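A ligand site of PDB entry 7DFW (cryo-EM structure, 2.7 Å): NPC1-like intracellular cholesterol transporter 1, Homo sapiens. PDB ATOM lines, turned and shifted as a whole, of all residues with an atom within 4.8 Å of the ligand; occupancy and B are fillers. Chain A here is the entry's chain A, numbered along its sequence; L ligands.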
ATOM      1  N   TYR A 646     -34.158  31.154  16.408  1.00  0.00           N
ATOM      2  CA  TYR A 646     -33.307  30.071  16.911  1.00  0.00           C
ATOM      3  C   TYR A 646     -32.235  29.679  15.902  1.00  0.00           C
ATOM      4  O   TYR A 646     -31.076  29.488  16.259  1.00  0.00           O
ATOM      5  CB  TYR A 646     -34.155  28.854  17.282  1.00  0.00           C
ATOM      6  CG  TYR A 646     -33.311  27.683  17.705  1.00  0.00           C
ATOM      7  CD1 TYR A 646     -32.453  27.770  18.785  1.00  0.00           C
ATOM      8  CD2 TYR A 646     -33.358  26.482  16.994  1.00  0.00           C
ATOM      9  CE1 TYR A 646     -31.665  26.696  19.177  1.00  0.00           C
ATOM     10  CE2 TYR A 646     -32.573  25.401  17.374  1.00  0.00           C
ATOM     11  CZ  TYR A 646     -31.730  25.519  18.464  1.00  0.00           C
ATOM     12  OH  TYR A 646     -30.953  24.460  18.840  1.00  0.00           O
ATOM     13  N   LEU A 649     -28.774  32.047  15.592  1.00  0.00           N
ATOM     14  CA  LEU A 649     -28.164  32.173  16.900  1.00  0.00           C
ATOM     15  C   LEU A 649     -27.508  30.878  17.331  1.00  0.00           C
ATOM     16  O   LEU A 649     -26.534  30.920  18.101  1.00  0.00           O
ATOM     17  CB  LEU A 649     -29.207  32.586  17.939  1.00  0.00           C
ATOM     18  CG  LEU A 649     -29.593  34.063  17.965  1.00  0.00           C
ATOM     19  CD1 LEU A 649     -30.460  34.364  19.178  1.00  0.00           C
ATOM     20  CD2 LEU A 649     -28.361  34.943  17.974  1.00  0.00           C
ATOM     21  N   ALA A 650     -28.004  29.749  16.849  1.00  0.00           N
ATOM     22  CA  ALA A 650     -27.364  28.454  17.002  1.00  0.00           C
ATOM     23  C   ALA A 650     -26.450  28.117  15.836  1.00  0.00           C
ATOM     24  O   ALA A 650     -25.779  27.074  15.882  1.00  0.00           O
ATOM     25  CB  ALA A 650     -28.413  27.359  17.165  1.00  0.00           C
ATOM     26  N   LEU A 651     -26.403  28.946  14.800  1.00  0.00           N
ATOM     27  CA  LEU A 651     -25.568  28.713  13.638  1.00  0.00           C
ATOM     28  C   LEU A 651     -24.530  29.799  13.424  1.00  0.00           C
ATOM     29  O   LEU A 651     -23.874  29.831  12.381  1.00  0.00           O
ATOM     30  CB  LEU A 651     -26.426  28.565  12.390  1.00  0.00           C
ATOM     31  CG  LEU A 651     -27.219  27.273  12.217  1.00  0.00           C
ATOM     32  CD1 LEU A 651     -28.180  27.393  11.054  1.00  0.00           C
ATOM     33  CD2 LEU A 651     -26.288  26.090  12.010  1.00  0.00           C
ATOM     34  N   GLY A 652     -24.365  30.709  14.385  1.00  0.00           N
ATOM     35  CA  GLY A 652     -23.413  31.793  14.258  1.00  0.00           C
ATOM     36  C   GLY A 652     -22.037  31.400  14.741  1.00  0.00           C
ATOM     37  O   GLY A 652     -21.785  30.288  15.199  1.00  0.00           O
ATOM     38  N   SER A 653     -21.107  32.360  14.633  1.00  0.00           N
ATOM     39  CA  SER A 653     -19.720  32.162  15.051  1.00  0.00           C
ATOM     40  C   SER A 653     -19.348  33.325  15.967  1.00  0.00           C
ATOM     41  O   SER A 653     -19.057  34.432  15.505  1.00  0.00           O
ATOM     42  CB  SER A 653     -18.792  32.076  13.853  1.00  0.00           C
ATOM     43  OG  SER A 653     -18.824  30.786  13.276  1.00  0.00           O
ATOM     44  N   TYR A 654     -19.353  33.058  17.270  1.00  0.00           N
ATOM     45  CA  TYR A 654     -19.120  34.056  18.310  1.00  0.00           C
ATOM     46  C   TYR A 654     -17.668  34.078  18.763  1.00  0.00           C
ATOM     47  O   TYR A 654     -17.350  33.956  19.946  1.00  0.00           O
ATOM     48  CB  TYR A 654     -20.065  33.812  19.473  1.00  0.00           C
ATOM     49  CG  TYR A 654     -21.505  33.668  19.055  1.00  0.00           C
ATOM     50  CD1 TYR A 654     -22.291  34.789  18.797  1.00  0.00           C
ATOM     51  CD2 TYR A 654     -22.093  32.400  18.913  1.00  0.00           C
ATOM     52  CE1 TYR A 654     -23.610  34.663  18.402  1.00  0.00           C
ATOM     53  CE2 TYR A 654     -23.398  32.265  18.493  1.00  0.00           C
ATOM     54  CZ  TYR A 654     -24.158  33.399  18.254  1.00  0.00           C
ATOM     55  OH  TYR A 654     -25.458  33.259  17.863  1.00  0.00           O
ATOM     56  N   LEU A 719     -24.785  22.492   9.629  1.00  0.00           N
ATOM     57  CA  LEU A 719     -23.839  22.167  10.689  1.00  0.00           C
ATOM     58  C   LEU A 719     -22.743  21.227  10.184  1.00  0.00           C
ATOM     59  O   LEU A 719     -21.570  21.383  10.548  1.00  0.00           O
ATOM     60  CB  LEU A 719     -24.610  21.574  11.863  1.00  0.00           C
ATOM     61  CG  LEU A 719     -23.915  21.283  13.182  1.00  0.00           C
ATOM     62  CD1 LEU A 719     -23.412  22.581  13.750  1.00  0.00           C
ATOM     63  CD2 LEU A 719     -24.914  20.657  14.119  1.00  0.00           C
ATOM     64  N   GLN A 722     -20.411  23.444   8.257  1.00  0.00           N
ATOM     65  CA  GLN A 722     -19.514  24.214   9.111  1.00  0.00           C
ATOM     66  C   GLN A 722     -18.433  23.358   9.745  1.00  0.00           C
ATOM     67  O   GLN A 722     -17.320  23.848   9.963  1.00  0.00           O
ATOM     68  CB  GLN A 722     -20.314  24.927  10.201  1.00  0.00           C
ATOM     69  CG  GLN A 722     -21.191  26.057   9.692  1.00  0.00           C
ATOM     70  CD  GLN A 722     -21.798  26.868  10.810  1.00  0.00           C
ATOM     71  OE1 GLN A 722     -21.701  26.498  11.970  1.00  0.00           O
ATOM     72  NE2 GLN A 722     -22.423  27.972  10.447  1.00  0.00           N
ATOM     73  N   GLY A 826     -16.400  25.677  18.783  1.00  0.00           N
ATOM     74  CA  GLY A 826     -17.666  26.091  19.332  1.00  0.00           C
ATOM     75  C   GLY A 826     -17.834  25.680  20.779  1.00  0.00           C
ATOM     76  O   GLY A 826     -16.905  25.309  21.481  1.00  0.00           O
ATOM     77  N   LEU A 827     -19.094  25.753  21.214  1.00  0.00           N
ATOM     78  CA  LEU A 827     -19.489  25.465  22.582  1.00  0.00           C
ATOM     79  C   LEU A 827     -20.286  24.175  22.690  1.00  0.00           C
ATOM     80  O   LEU A 827     -20.057  23.375  23.602  1.00  0.00           O
ATOM     81  CB  LEU A 827     -20.325  26.613  23.127  1.00  0.00           C
ATOM     82  CG  LEU A 827     -19.675  27.977  23.310  1.00  0.00           C
ATOM     83  CD1 LEU A 827     -20.758  28.919  23.679  1.00  0.00           C
ATOM     84  CD2 LEU A 827     -18.618  27.951  24.383  1.00  0.00           C
ATOM     85  N   LEU A 828     -21.244  23.990  21.784  1.00  0.00           N
ATOM     86  CA  LEU A 828     -22.073  22.787  21.781  1.00  0.00           C
ATOM     87  C   LEU A 828     -21.247  21.551  21.447  1.00  0.00           C
ATOM     88  O   LEU A 828     -21.250  20.562  22.194  1.00  0.00           O
ATOM     89  CB  LEU A 828     -23.214  22.938  20.780  1.00  0.00           C
ATOM     90  CG  LEU A 828     -24.095  21.716  20.586  1.00  0.00           C
ATOM     91  CD1 LEU A 828     -24.893  21.432  21.839  1.00  0.00           C
ATOM     92  CD2 LEU A 828     -25.003  21.894  19.394  1.00  0.00           C
ATOM     93  N   LEU A 829     -20.535  21.589  20.323  1.00  0.00           N
ATOM     94  CA  LEU A 829     -19.768  20.430  19.902  1.00  0.00           C
ATOM     95  C   LEU A 829     -18.544  20.236  20.786  1.00  0.00           C
ATOM     96  O   LEU A 829     -18.267  19.127  21.260  1.00  0.00           O
ATOM     97  CB  LEU A 829     -19.348  20.577  18.438  1.00  0.00           C
ATOM     98  CG  LEU A 829     -18.215  19.659  18.003  1.00  0.00           C
ATOM     99  CD1 LEU A 829     -18.729  18.246  17.859  1.00  0.00           C
ATOM    100  CD2 LEU A 829     -17.616  20.149  16.704  1.00  0.00           C
ATOM    101  N   PHE A 832     -19.353  20.997  25.694  1.00  0.00           N
ATOM    102  CA  PHE A 832     -20.280  20.226  26.515  1.00  0.00           C
ATOM    103  C   PHE A 832     -20.284  18.753  26.133  1.00  0.00           C
ATOM    104  O   PHE A 832     -20.315  17.897  27.016  1.00  0.00           O
ATOM    105  CB  PHE A 832     -21.692  20.796  26.449  1.00  0.00           C
ATOM    106  CG  PHE A 832     -22.526  20.416  27.637  1.00  0.00           C
ATOM    107  CD1 PHE A 832     -22.504  21.203  28.783  1.00  0.00           C
ATOM    108  CD2 PHE A 832     -23.309  19.269  27.627  1.00  0.00           C
ATOM    109  CE1 PHE A 832     -23.257  20.856  29.891  1.00  0.00           C
ATOM    110  CE2 PHE A 832     -24.064  18.912  28.733  1.00  0.00           C
ATOM    111  CZ  PHE A 832     -24.034  19.711  29.860  1.00  0.00           C
ATOM    112  N   GLN A 833     -20.279  18.443  24.832  1.00  0.00           N
ATOM    113  CA  GLN A 833     -20.381  17.040  24.431  1.00  0.00           C
ATOM    114  C   GLN A 833     -19.095  16.277  24.706  1.00  0.00           C
ATOM    115  O   GLN A 833     -19.142  15.063  24.916  1.00  0.00           O
ATOM    116  CB  GLN A 833     -20.774  16.950  22.957  1.00  0.00           C
ATOM    117  CG  GLN A 833     -22.103  17.614  22.637  1.00  0.00           C
ATOM    118  CD  GLN A 833     -23.295  16.785  23.047  1.00  0.00           C
ATOM    119  OE1 GLN A 833     -23.177  15.588  23.303  1.00  0.00           O
ATOM    120  NE2 GLN A 833     -24.462  17.408  23.094  1.00  0.00           N
ATOM    121  N   TYR A 836     -19.992  15.890  28.372  1.00  0.00           N
ATOM    122  CA  TYR A 836     -21.202  15.103  28.566  1.00  0.00           C
ATOM    123  C   TYR A 836     -21.027  13.661  28.138  1.00  0.00           C
ATOM    124  O   TYR A 836     -21.566  12.758  28.769  1.00  0.00           O
ATOM    125  CB  TYR A 836     -22.368  15.741  27.796  1.00  0.00           C
ATOM    126  CG  TYR A 836     -23.525  14.835  27.468  1.00  0.00           C
ATOM    127  CD1 TYR A 836     -24.440  14.464  28.454  1.00  0.00           C
ATOM    128  CD2 TYR A 836     -23.732  14.373  26.174  1.00  0.00           C
ATOM    129  CE1 TYR A 836     -25.519  13.632  28.159  1.00  0.00           C
ATOM    130  CE2 TYR A 836     -24.803  13.542  25.867  1.00  0.00           C
ATOM    131  CZ  TYR A 836     -25.692  13.184  26.871  1.00  0.00           C
ATOM    132  OH  TYR A 836     -26.750  12.360  26.574  1.00  0.00           O
ATOM    133  N   PHE A1213     -29.465  16.848  18.800  1.00  0.00           N
ATOM    134  CA  PHE A1213     -30.065  17.659  19.854  1.00  0.00           C
ATOM    135  C   PHE A1213     -30.327  19.090  19.403  1.00  0.00           C
ATOM    136  O   PHE A1213     -31.395  19.645  19.678  1.00  0.00           O
ATOM    137  CB  PHE A1213     -29.165  17.658  21.095  1.00  0.00           C
ATOM    138  CG  PHE A1213     -29.589  18.647  22.146  1.00  0.00           C
ATOM    139  CD1 PHE A1213     -30.742  18.422  22.883  1.00  0.00           C
ATOM    140  CD2 PHE A1213     -28.850  19.800  22.392  1.00  0.00           C
ATOM    141  CE1 PHE A1213     -31.163  19.334  23.844  1.00  0.00           C
ATOM    142  CE2 PHE A1213     -29.261  20.711  23.352  1.00  0.00           C
ATOM    143  CZ  PHE A1213     -30.408  20.477  24.076  1.00  0.00           C
ATOM    144  N   ALA A1214     -29.374  19.700  18.710  1.00  0.00           N
ATOM    145  CA  ALA A1214     -29.540  21.100  18.349  1.00  0.00           C
ATOM    146  C   ALA A1214     -30.541  21.272  17.214  1.00  0.00           C
ATOM    147  O   ALA A1214     -31.239  22.293  17.148  1.00  0.00           O
ATOM    148  CB  ALA A1214     -28.181  21.707  17.988  1.00  0.00           C
ATOM    149  N   MET A1218     -34.618  20.500  18.976  1.00  0.00           N
ATOM    150  CA  MET A1218     -34.866  21.908  19.264  1.00  0.00           C
ATOM    151  C   MET A1218     -35.736  22.616  18.240  1.00  0.00           C
ATOM    152  O   MET A1218     -36.360  23.630  18.595  1.00  0.00           O
ATOM    153  CB  MET A1218     -33.558  22.678  19.413  1.00  0.00           C
ATOM    154  CG  MET A1218     -32.722  22.267  20.589  1.00  0.00           C
ATOM    155  SD  MET A1218     -33.599  22.541  22.129  1.00  0.00           S
ATOM    156  CE  MET A1218     -33.633  24.328  22.179  1.00  0.00           C
ATOM    157  N   LEU A1221     -39.573  21.976  19.230  1.00  0.00           N
ATOM    158  CA  LEU A1221     -40.089  22.586  20.466  1.00  0.00           C
ATOM    159  C   LEU A1221     -40.978  23.809  20.248  1.00  0.00           C
ATOM    160  O   LEU A1221     -42.013  23.896  20.916  1.00  0.00           O
ATOM    161  CB  LEU A1221     -38.931  22.917  21.409  1.00  0.00           C
ATOM    162  CG  LEU A1221     -38.199  21.699  21.967  1.00  0.00           C
ATOM    163  CD1 LEU A1221     -37.003  22.129  22.780  1.00  0.00           C
ATOM    164  CD2 LEU A1221     -39.143  20.857  22.797  1.00  0.00           C
ATOM    165  N   LEU A1251     -36.022  12.043  21.966  1.00  0.00           N
ATOM    166  CA  LEU A1251     -34.752  12.612  22.401  1.00  0.00           C
ATOM    167  C   LEU A1251     -34.085  11.764  23.473  1.00  0.00           C
ATOM    168  O   LEU A1251     -32.872  11.563  23.444  1.00  0.00           O
ATOM    169  CB  LEU A1251     -34.975  14.039  22.906  1.00  0.00           C
ATOM    170  CG  LEU A1251     -33.761  14.744  23.493  1.00  0.00           C
ATOM    171  CD1 LEU A1251     -32.785  15.114  22.403  1.00  0.00           C
ATOM    172  CD2 LEU A1251     -34.190  15.968  24.273  1.00  0.00           C
ATOM    173  N   LEU A1255     -30.466  10.049  22.555  1.00  0.00           N
ATOM    174  CA  LEU A1255     -29.229  10.559  23.118  1.00  0.00           C
ATOM    175  C   LEU A1255     -28.795   9.873  24.411  1.00  0.00           C
ATOM    176  O   LEU A1255     -27.697  10.154  24.887  1.00  0.00           O
ATOM    177  CB  LEU A1255     -29.349  12.066  23.373  1.00  0.00           C
ATOM    178  CG  LEU A1255     -28.981  12.970  22.202  1.00  0.00           C
ATOM    179  CD1 LEU A1255     -30.043  12.908  21.111  1.00  0.00           C
ATOM    180  CD2 LEU A1255     -28.798  14.386  22.685  1.00  0.00           C
ATOM    181  N   VAL A1256     -29.618   9.004  24.996  1.00  0.00           N
ATOM    182  CA  VAL A1256     -29.222   8.391  26.259  1.00  0.00           C
ATOM    183  C   VAL A1256     -29.179   6.873  26.139  1.00  0.00           C
ATOM    184  O   VAL A1256     -28.352   6.213  26.767  1.00  0.00           O
ATOM    185  CB  VAL A1256     -30.174   8.825  27.379  1.00  0.00           C
ATOM    186  CG1 VAL A1256     -29.835   8.113  28.673  1.00  0.00           C
ATOM    187  CG2 VAL A1256     -30.114  10.315  27.568  1.00  0.00           C
HETATM  188  C1  LIG L   1     -19.648  27.284  15.267  1.00  0.00           C
HETATM  189  N1  LIG L   1     -21.449  25.724  14.697  1.00  0.00           N
HETATM  190  O1  LIG L   1     -19.187  28.241  15.936  1.00  0.00           O
HETATM  191  C2  LIG L   1     -24.160  27.414  22.533  1.00  0.00           C
HETATM  192  C3  LIG L   1     -24.332  27.193  21.013  1.00  0.00           C
HETATM  193  C4  LIG L   1     -23.498  28.171  20.211  1.00  0.00           C
HETATM  194  C5  LIG L   1     -21.159  27.045  15.214  1.00  0.00           C
HETATM  195  C6  LIG L   1     -21.773  27.201  16.600  1.00  0.00           C
HETATM  196  O2  LIG L   1     -20.877  26.775  17.576  1.00  0.00           O
HETATM  197  P1  LIG L   1     -21.354  27.024  19.123  1.00  0.00           P
HETATM  198  O3  LIG L   1     -21.187  25.821  19.929  1.00  0.00           O
HETATM  199  O4  LIG L   1     -20.455  27.951  19.792  1.00  0.00           O
HETATM  200  O5  LIG L   1     -22.930  27.518  19.112  1.00  0.00           O
HETATM  201  C7  LIG L   1     -24.279  25.853  24.372  1.00  0.00           C
HETATM  202  O6  LIG L   1     -23.734  26.490  25.198  1.00  0.00           O
HETATM  203  O7  LIG L   1     -24.904  26.493  23.279  1.00  0.00           O
HETATM  204  C8  LIG L   1     -24.341  24.327  24.498  1.00  0.00           C
HETATM  205  C9  LIG L   1     -25.356  23.915  25.575  1.00  0.00           C
HETATM  206  C10 LIG L   1     -26.062  22.598  25.237  1.00  0.00           C
HETATM  207  C11 LIG L   1     -27.089  22.248  26.319  1.00  0.00           C
HETATM  208  C12 LIG L   1     -26.882  20.909  27.048  1.00  0.00           C
HETATM  209  C13 LIG L   1     -27.575  19.767  26.308  1.00  0.00           C
HETATM  210  C14 LIG L   1     -27.262  18.401  26.920  1.00  0.00           C
HETATM  211  C15 LIG L   1     -28.032  17.289  26.189  1.00  0.00           C
HETATM  212  C16 LIG L   1     -28.960  16.546  27.141  1.00  0.00           C
HETATM  213  C17 LIG L   1     -29.754  15.476  26.371  1.00  0.00           C
HETATM  214  C18 LIG L   1     -30.846  14.845  27.251  1.00  0.00           C
HETATM  215  C19 LIG L   1     -30.294  13.937  28.352  1.00  0.00           C
HETATM  216  C20 LIG L   1     -30.476  14.590  29.735  1.00  0.00           C
HETATM  217  C21 LIG L   1     -29.848  13.759  30.860  1.00  0.00           C
HETATM  218  C22 LIG L   1     -30.754  12.610  31.307  1.00  0.00           C
HETATM  219  C23 LIG L   1     -30.132  11.872  32.493  1.00  0.00           C
HETATM  220  C24 LIG L   1     -30.061  10.370  32.196  1.00  0.00           C
HETATM  221  O8  LIG L   1     -25.656  27.415  20.630  1.00  0.00           O
HETATM  222  C25 LIG L   1     -26.391  26.267  20.352  1.00  0.00           C
HETATM  223  C26 LIG L   1     -27.253  25.700  21.464  1.00  0.00           C
HETATM  224  C27 LIG L   1     -28.682  25.413  21.034  1.00  0.00           C
HETATM  225  C28 LIG L   1     -29.414  24.504  22.041  1.00  0.00           C
HETATM  226  C29 LIG L   1     -29.523  25.131  23.447  1.00  0.00           C
HETATM  227  C30 LIG L   1     -30.887  24.925  24.091  1.00  0.00           C
HETATM  228  C31 LIG L   1     -30.804  25.192  25.605  1.00  0.00           C
HETATM  229  C32 LIG L   1     -30.560  23.962  26.496  1.00  0.00           C
HETATM  230  C33 LIG L   1     -31.325  24.082  27.818  1.00  0.00           C
HETATM  231  O9  LIG L   1     -26.343  25.754  19.282  1.00  0.00           O
HETATM  232  C34 LIG L   1     -32.818  23.746  27.710  1.00  0.00           C
HETATM  233  C35 LIG L   1     -33.672  24.929  28.193  1.00  0.00           C
HETATM  234  C36 LIG L   1     -35.186  24.670  28.189  1.00  0.00           C
HETATM  235  C37 LIG L   1     -35.774  24.452  26.795  1.00  0.00           C
HETATM  236  C38 LIG L   1     -35.895  22.969  26.401  1.00  0.00           C
HETATM  237  O10 LIG L   1     -18.863  26.519  14.645  1.00  0.00           O
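O of Gly 652 lies close to O1 of the ligand. Residues that only touch the ligand: Tyr 646, Ala 650, Ser 653, Leu 719, Gly 826, Phe 832, Phe 1213, Met 1218, Leu 1221, Leu 1255 and Val 1256. Hydrophobic or aromatic side chains that line the ligand: Tyr 646, Ala 650, Leu 719, Leu 827, Leu 828, Phe 832, Phe 1213, Met 1218, Leu 1221, Leu 1255 and Val 1256. The nearest printed residue that does not touch the ligand is Tyr 836 (4.3 Å).
The backbone carbonyl oxygen (O) of Leu 827 lies within hydrogen-bond range of the backbone NH (N) of Phe 832 (3.2 Å). NE2 of Gln 722 is in hydrogen-bond range of O of Leu 651. The backbone carbonyl oxygen (O) of Ala 1214 is in hydrogen-bond range of the side-chain hydroxyl (OH) of Tyr 646 (2.8 Å). The backbone NH of Met 1218 lies close to the backbone carbonyl oxygen of Phe 1213, at 3.4 Å. The backbone carbonyl oxygen (O) of Leu 1255 lies within hydrogen-bond range of the side-chain hydroxyl (OH) of Tyr 836 (2.9 Å).
N of Leu 827 lies within hydrogen-bond range of O3 of the ligand (2.5 Å). N of Leu 828 lies within hydrogen-bond range of O3 of the ligand (2.6 Å). N1 of the ligand is in hydrogen-bond range of OE1 of Gln 722, at 2.8 Å.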
